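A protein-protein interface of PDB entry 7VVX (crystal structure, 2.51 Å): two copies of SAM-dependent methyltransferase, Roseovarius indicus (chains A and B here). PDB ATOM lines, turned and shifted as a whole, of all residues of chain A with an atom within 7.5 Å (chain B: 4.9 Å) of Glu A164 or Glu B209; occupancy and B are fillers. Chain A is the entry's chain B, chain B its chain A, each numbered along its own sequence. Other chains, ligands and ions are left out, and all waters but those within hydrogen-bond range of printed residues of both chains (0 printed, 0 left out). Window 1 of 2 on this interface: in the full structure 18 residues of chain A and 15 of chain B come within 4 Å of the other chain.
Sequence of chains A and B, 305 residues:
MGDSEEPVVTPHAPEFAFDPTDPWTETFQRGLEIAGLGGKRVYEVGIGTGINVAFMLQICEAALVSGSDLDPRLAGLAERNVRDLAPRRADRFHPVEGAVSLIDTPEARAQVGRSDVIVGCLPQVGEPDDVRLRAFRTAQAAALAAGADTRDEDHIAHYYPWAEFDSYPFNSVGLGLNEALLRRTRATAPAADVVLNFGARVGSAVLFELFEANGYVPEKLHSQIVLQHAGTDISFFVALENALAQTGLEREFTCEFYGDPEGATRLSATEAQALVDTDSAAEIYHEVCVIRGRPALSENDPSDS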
ATOM      1  N   SER A 101     -20.769   7.484 -22.592  1.00  0.00           N
ATOM      2  CA  SER A 101     -20.145   7.542 -21.278  1.00  0.00           C
ATOM      3  C   SER A 101     -19.037   8.597 -21.323  1.00  0.00           C
ATOM      4  O   SER A 101     -18.164   8.549 -22.197  1.00  0.00           O
ATOM      5  CB  SER A 101     -19.605   6.173 -20.871  1.00  0.00           C
ATOM      6  OG  SER A 101     -19.277   6.159 -19.493  1.00  0.00           O
ATOM      7  N   LEU A 102     -19.104   9.572 -20.408  1.00  0.00           N
ATOM      8  CA  LEU A 102     -18.168  10.695 -20.321  1.00  0.00           C
ATOM      9  C   LEU A 102     -18.168  11.390 -21.676  1.00  0.00           C
ATOM     10  O   LEU A 102     -19.211  11.896 -22.097  1.00  0.00           O
ATOM     11  CB  LEU A 102     -16.785  10.204 -19.901  1.00  0.00           C
ATOM     12  CG  LEU A 102     -16.825   9.728 -18.447  1.00  0.00           C
ATOM     13  CD1 LEU A 102     -15.433   9.478 -17.918  1.00  0.00           C
ATOM     14  CD2 LEU A 102     -17.549  10.728 -17.577  1.00  0.00           C
ATOM     15  N   ASP A 104     -16.806   9.701 -24.554  1.00  0.00           N
ATOM     16  CA  ASP A 104     -16.133   8.611 -25.267  1.00  0.00           C
ATOM     17  C   ASP A 104     -16.820   8.200 -26.569  1.00  0.00           C
ATOM     18  O   ASP A 104     -17.046   7.013 -26.812  1.00  0.00           O
ATOM     19  CB  ASP A 104     -15.990   7.414 -24.339  1.00  0.00           C
ATOM     20  CG  ASP A 104     -15.275   7.760 -23.047  1.00  0.00           C
ATOM     21  OD1 ASP A 104     -14.803   8.911 -22.912  1.00  0.00           O
ATOM     22  OD2 ASP A 104     -15.183   6.882 -22.158  1.00  0.00           O
ATOM     23  N   TYR A 160     -22.606  -0.801 -14.827  1.00  0.00           N
ATOM     24  CA  TYR A 160     -22.800   0.276 -15.809  1.00  0.00           C
ATOM     25  C   TYR A 160     -23.318   1.644 -15.309  1.00  0.00           C
ATOM     26  O   TYR A 160     -24.520   1.896 -15.407  1.00  0.00           O
ATOM     27  CB  TYR A 160     -23.623  -0.215 -17.010  1.00  0.00           C
ATOM     28  CG  TYR A 160     -23.196   0.382 -18.331  1.00  0.00           C
ATOM     29  CD1 TYR A 160     -22.027   1.124 -18.434  1.00  0.00           C
ATOM     30  CD2 TYR A 160     -23.962   0.206 -19.476  1.00  0.00           C
ATOM     31  CE1 TYR A 160     -21.633   1.673 -19.640  1.00  0.00           C
ATOM     32  CE2 TYR A 160     -23.576   0.750 -20.685  1.00  0.00           C
ATOM     33  CZ  TYR A 160     -22.411   1.483 -20.761  1.00  0.00           C
ATOM     34  OH  TYR A 160     -22.023   2.027 -21.964  1.00  0.00           O
ATOM     35  N   PRO A 161     -22.405   2.506 -14.904  1.00  0.00           N
ATOM     36  CA  PRO A 161     -20.999   2.113 -14.919  1.00  0.00           C
ATOM     37  C   PRO A 161     -20.305   2.537 -13.658  1.00  0.00           C
ATOM     38  O   PRO A 161     -20.740   3.474 -12.988  1.00  0.00           O
ATOM     39  CB  PRO A 161     -20.437   2.890 -16.111  1.00  0.00           C
ATOM     40  CG  PRO A 161     -21.300   4.101 -16.201  1.00  0.00           C
ATOM     41  CD  PRO A 161     -22.673   3.655 -15.787  1.00  0.00           C
ATOM     42  N   TRP A 162     -19.216   1.859 -13.309  1.00  0.00           N
ATOM     43  CA  TRP A 162     -18.492   2.215 -12.093  1.00  0.00           C
ATOM     44  C   TRP A 162     -17.157   1.495 -11.902  1.00  0.00           C
ATOM     45  O   TRP A 162     -16.217   2.071 -11.353  1.00  0.00           O
ATOM     46  CB  TRP A 162     -19.379   1.989 -10.865  1.00  0.00           C
ATOM     47  CG  TRP A 162     -20.121   0.688 -10.892  1.00  0.00           C
ATOM     48  CD1 TRP A 162     -21.104   0.323 -11.765  1.00  0.00           C
ATOM     49  CD2 TRP A 162     -19.941  -0.422 -10.004  1.00  0.00           C
ATOM     50  NE1 TRP A 162     -21.546  -0.946 -11.477  1.00  0.00           N
ATOM     51  CE2 TRP A 162     -20.849  -1.424 -10.400  1.00  0.00           C
ATOM     52  CE3 TRP A 162     -19.101  -0.666  -8.913  1.00  0.00           C
ATOM     53  CZ2 TRP A 162     -20.940  -2.650  -9.744  1.00  0.00           C
ATOM     54  CZ3 TRP A 162     -19.193  -1.883  -8.264  1.00  0.00           C
ATOM     55  CH2 TRP A 162     -20.105  -2.860  -8.681  1.00  0.00           C
ATOM     56  N   ALA A 163     -17.067   0.245 -12.344  1.00  0.00           N
ATOM     57  CA  ALA A 163     -15.831  -0.500 -12.174  1.00  0.00           C
ATOM     58  C   ALA A 163     -14.564  -0.138 -12.899  1.00  0.00           C
ATOM     59  O   ALA A 163     -13.506  -0.425 -12.436  1.00  0.00           O
ATOM     60  CB  ALA A 163     -16.107  -1.942 -12.413  1.00  0.00           C
ATOM     61  N   GLU A 164     -14.659   0.458 -14.050  1.00  0.00           N
ATOM     62  CA  GLU A 164     -13.482   0.803 -14.768  1.00  0.00           C
ATOM     63  C   GLU A 164     -12.851   1.985 -14.168  1.00  0.00           C
ATOM     64  O   GLU A 164     -11.746   2.254 -14.402  1.00  0.00           O
ATOM     65  CB  GLU A 164     -13.813   1.051 -16.192  1.00  0.00           C
ATOM     66  CG  GLU A 164     -14.746   2.177 -16.380  1.00  0.00           C
ATOM     67  CD  GLU A 164     -16.109   1.694 -16.681  1.00  0.00           C
ATOM     68  OE1 GLU A 164     -16.763   2.225 -17.574  1.00  0.00           O
ATOM     69  OE2 GLU A 164     -16.509   0.767 -16.008  1.00  0.00           O
ATOM     70  N   PHE A 165     -13.569   2.690 -13.358  1.00  0.00           N
ATOM     71  CA  PHE A 165     -13.001   3.863 -12.715  1.00  0.00           C
ATOM     72  C   PHE A 165     -12.463   3.556 -11.332  1.00  0.00           C
ATOM     73  O   PHE A 165     -12.093   4.479 -10.599  1.00  0.00           O
ATOM     74  CB  PHE A 165     -14.038   4.980 -12.664  1.00  0.00           C
ATOM     75  CG  PHE A 165     -14.697   5.216 -13.983  1.00  0.00           C
ATOM     76  CD1 PHE A 165     -13.972   5.707 -15.048  1.00  0.00           C
ATOM     77  CD2 PHE A 165     -16.023   4.874 -14.190  1.00  0.00           C
ATOM     78  CE1 PHE A 165     -14.562   5.899 -16.285  1.00  0.00           C
ATOM     79  CE2 PHE A 165     -16.620   5.067 -15.435  1.00  0.00           C
ATOM     80  CZ  PHE A 165     -15.882   5.584 -16.476  1.00  0.00           C
ATOM     81  N   ASP A 166     -12.373   2.275 -10.979  1.00  0.00           N
ATOM     82  CA  ASP A 166     -11.939   1.904  -9.640  1.00  0.00           C
ATOM     83  C   ASP A 166     -10.454   2.150  -9.434  1.00  0.00           C
ATOM     84  O   ASP A 166     -10.020   2.317  -8.302  1.00  0.00           O
ATOM     85  CB  ASP A 166     -12.278   0.432  -9.364  1.00  0.00           C
ATOM     86  CG  ASP A 166     -12.442   0.123  -7.868  1.00  0.00           C
ATOM     87  OD1 ASP A 166     -13.316   0.741  -7.218  1.00  0.00           O
ATOM     88  OD2 ASP A 166     -11.709  -0.754  -7.345  1.00  0.00           O
ATOM     89  N   SER A 167      -9.652   2.174 -10.495  1.00  0.00           N
ATOM     90  CA  SER A 167      -8.208   2.334 -10.322  1.00  0.00           C
ATOM     91  C   SER A 167      -7.771   3.777 -10.057  1.00  0.00           C
ATOM     92  O   SER A 167      -6.638   3.987  -9.592  1.00  0.00           O
ATOM     93  CB  SER A 167      -7.478   1.823 -11.562  1.00  0.00           C
ATOM     94  OG  SER A 167      -8.167   2.238 -12.723  1.00  0.00           O
ATOM     95  N   TYR A 168      -8.623   4.765 -10.350  1.00  0.00           N
ATOM     96  CA  TYR A 168      -8.205   6.160 -10.290  1.00  0.00           C
ATOM     97  C   TYR A 168      -7.794   6.532  -8.871  1.00  0.00           C
ATOM     98  O   TYR A 168      -8.548   6.275  -7.933  1.00  0.00           O
ATOM     99  CB  TYR A 168      -9.325   7.080 -10.772  1.00  0.00           C
ATOM    100  CG  TYR A 168      -9.420   7.077 -12.259  1.00  0.00           C
ATOM    101  CD1 TYR A 168      -8.649   7.922 -13.005  1.00  0.00           C
ATOM    102  CD2 TYR A 168     -10.230   6.169 -12.922  1.00  0.00           C
ATOM    103  CE1 TYR A 168      -8.697   7.900 -14.368  1.00  0.00           C
ATOM    104  CE2 TYR A 168     -10.289   6.137 -14.297  1.00  0.00           C
ATOM    105  CZ  TYR A 168      -9.514   7.009 -15.012  1.00  0.00           C
ATOM    106  OH  TYR A 168      -9.535   7.007 -16.381  1.00  0.00           O
ATOM    107  N   GLY A 176     -13.549   9.105  -8.424  1.00  0.00           N
ATOM    108  CA  GLY A 176     -12.967   8.410  -9.571  1.00  0.00           C
ATOM    109  C   GLY A 176     -13.544   8.804 -10.921  1.00  0.00           C
ATOM    110  O   GLY A 176     -12.808   9.017 -11.881  1.00  0.00           O
ATOM    111  N   LEU A 177     -14.869   8.858 -11.037  1.00  0.00           N
ATOM    112  CA  LEU A 177     -15.449   9.245 -12.321  1.00  0.00           C
ATOM    113  C   LEU A 177     -15.056  10.679 -12.672  1.00  0.00           C
ATOM    114  O   LEU A 177     -14.709  10.980 -13.827  1.00  0.00           O
ATOM    115  CB  LEU A 177     -16.971   9.073 -12.291  1.00  0.00           C
ATOM    116  CG  LEU A 177     -17.772   9.366 -13.555  1.00  0.00           C
ATOM    117  CD1 LEU A 177     -17.327   8.480 -14.715  1.00  0.00           C
ATOM    118  CD2 LEU A 177     -19.243   9.123 -13.295  1.00  0.00           C
ATOM    119  N   GLU A 179     -12.276  12.215 -11.772  1.00  0.00           N
ATOM    120  CA  GLU A 179     -10.895  12.180 -12.250  1.00  0.00           C
ATOM    121  C   GLU A 179     -10.835  11.646 -13.674  1.00  0.00           C
ATOM    122  O   GLU A 179     -10.143  12.206 -14.539  1.00  0.00           O
ATOM    123  CB  GLU A 179     -10.016  11.327 -11.322  1.00  0.00           C
ATOM    124  CG  GLU A 179      -8.569  11.199 -11.826  1.00  0.00           C
ATOM    125  CD  GLU A 179      -7.547  10.859 -10.745  1.00  0.00           C
ATOM    126  OE1 GLU A 179      -7.867  10.048  -9.837  1.00  0.00           O
ATOM    127  OE2 GLU A 179      -6.409  11.407 -10.817  1.00  0.00           O
ATOM    128  N   ALA A 180     -11.565  10.557 -13.933  1.00  0.00           N
ATOM    129  CA  ALA A 180     -11.574   9.956 -15.260  1.00  0.00           C
ATOM    130  C   ALA A 180     -11.997  10.959 -16.315  1.00  0.00           C
ATOM    131  O   ALA A 180     -11.550  10.875 -17.460  1.00  0.00           O
ATOM    132  CB  ALA A 180     -12.501   8.740 -15.275  1.00  0.00           C
ATOM    133  N   LEU A 181     -12.865  11.904 -15.953  1.00  0.00           N
ATOM    134  CA  LEU A 181     -13.251  12.947 -16.893  1.00  0.00           C
ATOM    135  C   LEU A 181     -12.086  13.886 -17.157  1.00  0.00           C
ATOM    136  O   LEU A 181     -11.789  14.200 -18.315  1.00  0.00           O
ATOM    137  CB  LEU A 181     -14.457  13.729 -16.369  1.00  0.00           C
ATOM    138  CG  LEU A 181     -14.756  14.962 -17.234  1.00  0.00           C
ATOM    139  CD1 LEU A 181     -14.996  14.545 -18.692  1.00  0.00           C
ATOM    140  CD2 LEU A 181     -15.934  15.789 -16.699  1.00  0.00           C
ATOM    141  N   ARG A 183      -8.914  13.419 -17.048  1.00  0.00           N
ATOM    142  CA  ARG A 183      -7.931  12.822 -17.950  1.00  0.00           C
ATOM    143  C   ARG A 183      -8.371  12.956 -19.400  1.00  0.00           C
ATOM    144  O   ARG A 183      -7.541  13.167 -20.286  1.00  0.00           O
ATOM    145  CB  ARG A 183      -7.700  11.353 -17.626  1.00  0.00           C
ATOM    146  CG  ARG A 183      -7.395  11.084 -16.197  1.00  0.00           C
ATOM    147  CD  ARG A 183      -6.006  11.479 -15.851  1.00  0.00           C
ATOM    148  NE  ARG A 183      -5.695  11.064 -14.490  1.00  0.00           N
ATOM    149  CZ  ARG A 183      -5.132   9.903 -14.153  1.00  0.00           C
ATOM    150  NH1 ARG A 183      -4.784   9.005 -15.075  1.00  0.00           N
ATOM    151  NH2 ARG A 183      -4.908   9.640 -12.875  1.00  0.00           N
ATOM    152  N   ARG A 184      -9.672  12.847 -19.667  1.00  0.00           N
ATOM    153  CA  ARG A 184     -10.129  12.986 -21.046  1.00  0.00           C
ATOM    154  C   ARG A 184     -10.045  14.434 -21.528  1.00  0.00           C
ATOM    155  O   ARG A 184      -9.577  14.692 -22.642  1.00  0.00           O
ATOM    156  CB  ARG A 184     -11.549  12.448 -21.179  1.00  0.00           C
ATOM    157  CG  ARG A 184     -11.625  10.925 -21.106  1.00  0.00           C
ATOM    158  CD  ARG A 184     -12.913  10.487 -20.403  1.00  0.00           C
ATOM    159  NE  ARG A 184     -13.261   9.099 -20.680  1.00  0.00           N
ATOM    160  CZ  ARG A 184     -12.771   8.053 -20.027  1.00  0.00           C
ATOM    161  NH1 ARG A 184     -11.897   8.221 -19.045  1.00  0.00           N
ATOM    162  NH2 ARG A 184     -13.152   6.831 -20.366  1.00  0.00           N
ATOM    163  N   PHE B 170      -3.385   0.995 -12.651  1.00  0.00           N
ATOM    164  CA  PHE B 170      -3.788  -0.179 -13.403  1.00  0.00           C
ATOM    165  C   PHE B 170      -2.919  -1.383 -13.129  1.00  0.00           C
ATOM    166  O   PHE B 170      -3.077  -2.409 -13.800  1.00  0.00           O
ATOM    167  CB  PHE B 170      -3.805   0.142 -14.890  1.00  0.00           C
ATOM    168  CG  PHE B 170      -4.981   0.973 -15.284  1.00  0.00           C
ATOM    169  CD1 PHE B 170      -6.190   0.370 -15.636  1.00  0.00           C
ATOM    170  CD2 PHE B 170      -4.902   2.355 -15.264  1.00  0.00           C
ATOM    171  CE1 PHE B 170      -7.306   1.141 -15.985  1.00  0.00           C
ATOM    172  CE2 PHE B 170      -5.997   3.129 -15.606  1.00  0.00           C
ATOM    173  CZ  PHE B 170      -7.220   2.515 -15.958  1.00  0.00           C
ATOM    174  N   ALA B 205     -14.012  -2.810 -20.958  1.00  0.00           N
ATOM    175  CA  ALA B 205     -14.184  -1.443 -20.479  1.00  0.00           C
ATOM    176  C   ALA B 205     -12.949  -0.964 -19.736  1.00  0.00           C
ATOM    177  O   ALA B 205     -12.630   0.230 -19.759  1.00  0.00           O
ATOM    178  CB  ALA B 205     -15.406  -1.332 -19.561  1.00  0.00           C
ATOM    179  N   VAL B 206     -12.270  -1.877 -19.054  1.00  0.00           N
ATOM    180  CA  VAL B 206     -11.130  -1.520 -18.241  1.00  0.00           C
ATOM    181  C   VAL B 206      -9.881  -1.431 -19.097  1.00  0.00           C
ATOM    182  O   VAL B 206      -9.055  -0.531 -18.900  1.00  0.00           O
ATOM    183  CB  VAL B 206     -10.959  -2.528 -17.093  1.00  0.00           C
ATOM    184  CG1 VAL B 206     -10.774  -3.863 -17.666  1.00  0.00           C
ATOM    185  CG2 VAL B 206      -9.730  -2.186 -16.260  1.00  0.00           C
ATOM    186  N   LEU B 207      -9.727  -2.346 -20.062  1.00  0.00           N
ATOM    187  CA  LEU B 207      -8.634  -2.203 -21.007  1.00  0.00           C
ATOM    188  C   LEU B 207      -8.726  -0.859 -21.697  1.00  0.00           C
ATOM    189  O   LEU B 207      -7.722  -0.151 -21.823  1.00  0.00           O
ATOM    190  CB  LEU B 207      -8.656  -3.335 -22.027  1.00  0.00           C
ATOM    191  CG  LEU B 207      -8.399  -4.742 -21.479  1.00  0.00           C
ATOM    192  CD1 LEU B 207      -8.262  -5.742 -22.626  1.00  0.00           C
ATOM    193  CD2 LEU B 207      -7.202  -4.822 -20.549  1.00  0.00           C
ATOM    194  N   PHE B 208      -9.941  -0.457 -22.089  1.00  0.00           N
ATOM    195  CA  PHE B 208     -10.099   0.855 -22.693  1.00  0.00           C
ATOM    196  C   PHE B 208      -9.730   1.953 -21.713  1.00  0.00           C
ATOM    197  O   PHE B 208      -9.021   2.900 -22.076  1.00  0.00           O
ATOM    198  CB  PHE B 208     -11.510   1.034 -23.201  1.00  0.00           C
ATOM    199  CG  PHE B 208     -11.729   0.400 -24.516  1.00  0.00           C
ATOM    200  CD1 PHE B 208     -11.007  -0.736 -24.864  1.00  0.00           C
ATOM    201  CD2 PHE B 208     -12.624   0.941 -25.429  1.00  0.00           C
ATOM    202  CE1 PHE B 208     -11.185  -1.341 -26.093  1.00  0.00           C
ATOM    203  CE2 PHE B 208     -12.808   0.346 -26.666  1.00  0.00           C
ATOM    204  CZ  PHE B 208     -12.082  -0.799 -26.998  1.00  0.00           C
ATOM    205  N   GLU B 209     -10.160   1.820 -20.453  1.00  0.00           N
ATOM    206  CA  GLU B 209      -9.831   2.833 -19.465  1.00  0.00           C
ATOM    207  C   GLU B 209      -8.325   2.975 -19.264  1.00  0.00           C
ATOM    208  O   GLU B 209      -7.845   4.093 -19.014  1.00  0.00           O
ATOM    209  CB  GLU B 209     -10.519   2.530 -18.138  1.00  0.00           C
ATOM    210  CG  GLU B 209     -10.723   3.780 -17.282  1.00  0.00           C
ATOM    211  CD  GLU B 209     -11.457   4.903 -18.031  1.00  0.00           C
ATOM    212  OE1 GLU B 209     -12.238   4.589 -18.964  1.00  0.00           O
ATOM    213  OE2 GLU B 209     -11.259   6.102 -17.684  1.00  0.00           O
ATOM    214  N   LEU B 210      -7.561   1.874 -19.380  1.00  0.00           N
ATOM    215  CA  LEU B 210      -6.104   1.982 -19.313  1.00  0.00           C
ATOM    216  C   LEU B 210      -5.578   3.031 -20.296  1.00  0.00           C
ATOM    217  O   LEU B 210      -4.631   3.762 -19.990  1.00  0.00           O
ATOM    218  CB  LEU B 210      -5.454   0.622 -19.585  1.00  0.00           C
ATOM    219  CG  LEU B 210      -3.962   0.697 -19.960  1.00  0.00           C
ATOM    220  CD1 LEU B 210      -3.110   1.168 -18.791  1.00  0.00           C
ATOM    221  CD2 LEU B 210      -3.448  -0.617 -20.451  1.00  0.00           C
ATOM    222  N   PHE B 211      -6.203   3.134 -21.470  1.00  0.00           N
ATOM    223  CA  PHE B 211      -5.793   4.087 -22.495  1.00  0.00           C
ATOM    224  C   PHE B 211      -6.357   5.472 -22.229  1.00  0.00           C
ATOM    225  O   PHE B 211      -5.637   6.473 -22.308  1.00  0.00           O
ATOM    226  CB  PHE B 211      -6.251   3.608 -23.880  1.00  0.00           C
ATOM    227  CG  PHE B 211      -5.423   2.483 -24.437  1.00  0.00           C
ATOM    228  CD1 PHE B 211      -4.303   2.749 -25.215  1.00  0.00           C
ATOM    229  CD2 PHE B 211      -5.749   1.157 -24.157  1.00  0.00           C
ATOM    230  CE1 PHE B 211      -3.533   1.710 -25.722  1.00  0.00           C
ATOM    231  CE2 PHE B 211      -4.982   0.115 -24.660  1.00  0.00           C
ATOM    232  CZ  PHE B 211      -3.875   0.390 -25.446  1.00  0.00           C
ATOM    233  N   GLU B 212      -7.658   5.540 -21.950  1.00  0.00           N
ATOM    234  CA  GLU B 212      -8.294   6.816 -21.672  1.00  0.00           C
ATOM    235  C   GLU B 212      -7.647   7.503 -20.477  1.00  0.00           C
ATOM    236  O   GLU B 212      -7.514   8.730 -20.457  1.00  0.00           O
ATOM    237  CB  GLU B 212      -9.777   6.597 -21.415  1.00  0.00           C
ATOM    238  CG  GLU B 212     -10.498   5.972 -22.554  1.00  0.00           C
ATOM    239  CD  GLU B 212     -11.024   6.999 -23.532  1.00  0.00           C
ATOM    240  OE1 GLU B 212     -10.663   8.184 -23.404  1.00  0.00           O
ATOM    241  OE2 GLU B 212     -11.823   6.616 -24.421  1.00  0.00           O
ATOM    242  N   ALA B 213      -7.247   6.727 -19.466  1.00  0.00           N
ATOM    243  CA  ALA B 213      -6.594   7.317 -18.310  1.00  0.00           C
ATOM    244  C   ALA B 213      -5.267   7.966 -18.669  1.00  0.00           C
ATOM    245  O   ALA B 213      -4.768   8.766 -17.878  1.00  0.00           O
ATOM    246  CB  ALA B 213      -6.365   6.270 -17.211  1.00  0.00           C
ATOM    247  N   ASN B 214      -4.700   7.667 -19.843  1.00  0.00           N
ATOM    248  CA  ASN B 214      -3.328   8.056 -20.142  1.00  0.00           C
ATOM    249  C   ASN B 214      -3.205   8.763 -21.478  1.00  0.00           C
ATOM    250  O   ASN B 214      -2.174   8.669 -22.114  1.00  0.00           O
ATOM    251  CB  ASN B 214      -2.399   6.845 -20.088  1.00  0.00           C
ATOM    252  CG  ASN B 214      -2.225   6.324 -18.655  1.00  0.00           C
ATOM    253  OD1 ASN B 214      -1.576   6.973 -17.822  1.00  0.00           O
ATOM    254  ND2 ASN B 214      -2.825   5.170 -18.356  1.00  0.00           N
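The side-chain carboxylate (OE2) of Glu B209 lies within salt-bridge range of the guanidinium group (NH1) of Arg A184 (2.6 Å). The guanidinium group of Arg A184 lies within salt-bridge range of the side-chain carboxylate of Glu B212. The guanidinium group of Arg A183 sits at hydrogen-bond distance from the backbone carbonyl oxygen of Ala B213 (2.8 Å). OE2 of Glu B209 sits close to OH of Tyr A168 (2.3 Å).
Among the printed residues, merely in contact across the chains: Asp A104 with Glu B212, Glu A164 with Ala B205, Glu A164 with Glu B209, Phe A165 with Glu B209, Ser A167 with Phe B170, Tyr A168 with Ala B213, Ala A180 with Glu B209 and Arg A183 with Glu B212.
Hydrophobic or aromatic side chains of chain A within 4 Å of the printed part of chain B: Phe A165, Tyr A168 and Ala A180. Along chain A the printed residues that touch a printed residue of chain B span positions 104 to 184. Among the printed residues, 12 pairs touch across the chains. Among the printed residues, Asp or Glu carboxylates within 4 Å of a Lys or Arg side-chain nitrogen of the other chain: Arg A184 with Glu B209 and Arg A184 with Glu B212.
OD2 of Asp A104 lies within salt-bridge range of NH2 of Arg A184, 2.7 Å away. The side-chain carboxylate (OE2) of Glu A179 lies within salt-bridge range of the guanidinium group (NH2) of Arg A183. The guanidinium group (NH1) of Arg A184 lies within hydrogen-bond range of the backbone carbonyl oxygen (O) of Ala A180 (3.1 Å).
Of chain B, only Ala B205 and Glu B209 come within 4 Å of Glu A164. Glu B209 touches five residues of chain A. Printed residues of chain B within 4 Å of Tyr A168: Glu B209 (2.3 Å) and Ala B213 (3.4 Å). Printed residues of chain B within 4 Å of Ser A167: Phe B170 (3.4 Å). Of the printed residues of chain B, Ala A180 touches Glu B209. Of the printed residues of chain A, Ala B205 touches Glu A164 (3.8 Å). The nearest residue of chain A that does not touch Glu B209 is Asp A104 (4.9 Å). The nearest printed residue of chain B that does not touch Tyr A168 is Glu B212 (4.5 Å).
No position is printed for both chains. Of the 12 pairs that touch across the chains among the printed residues, none has its exchanged pair printed and touching as well.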
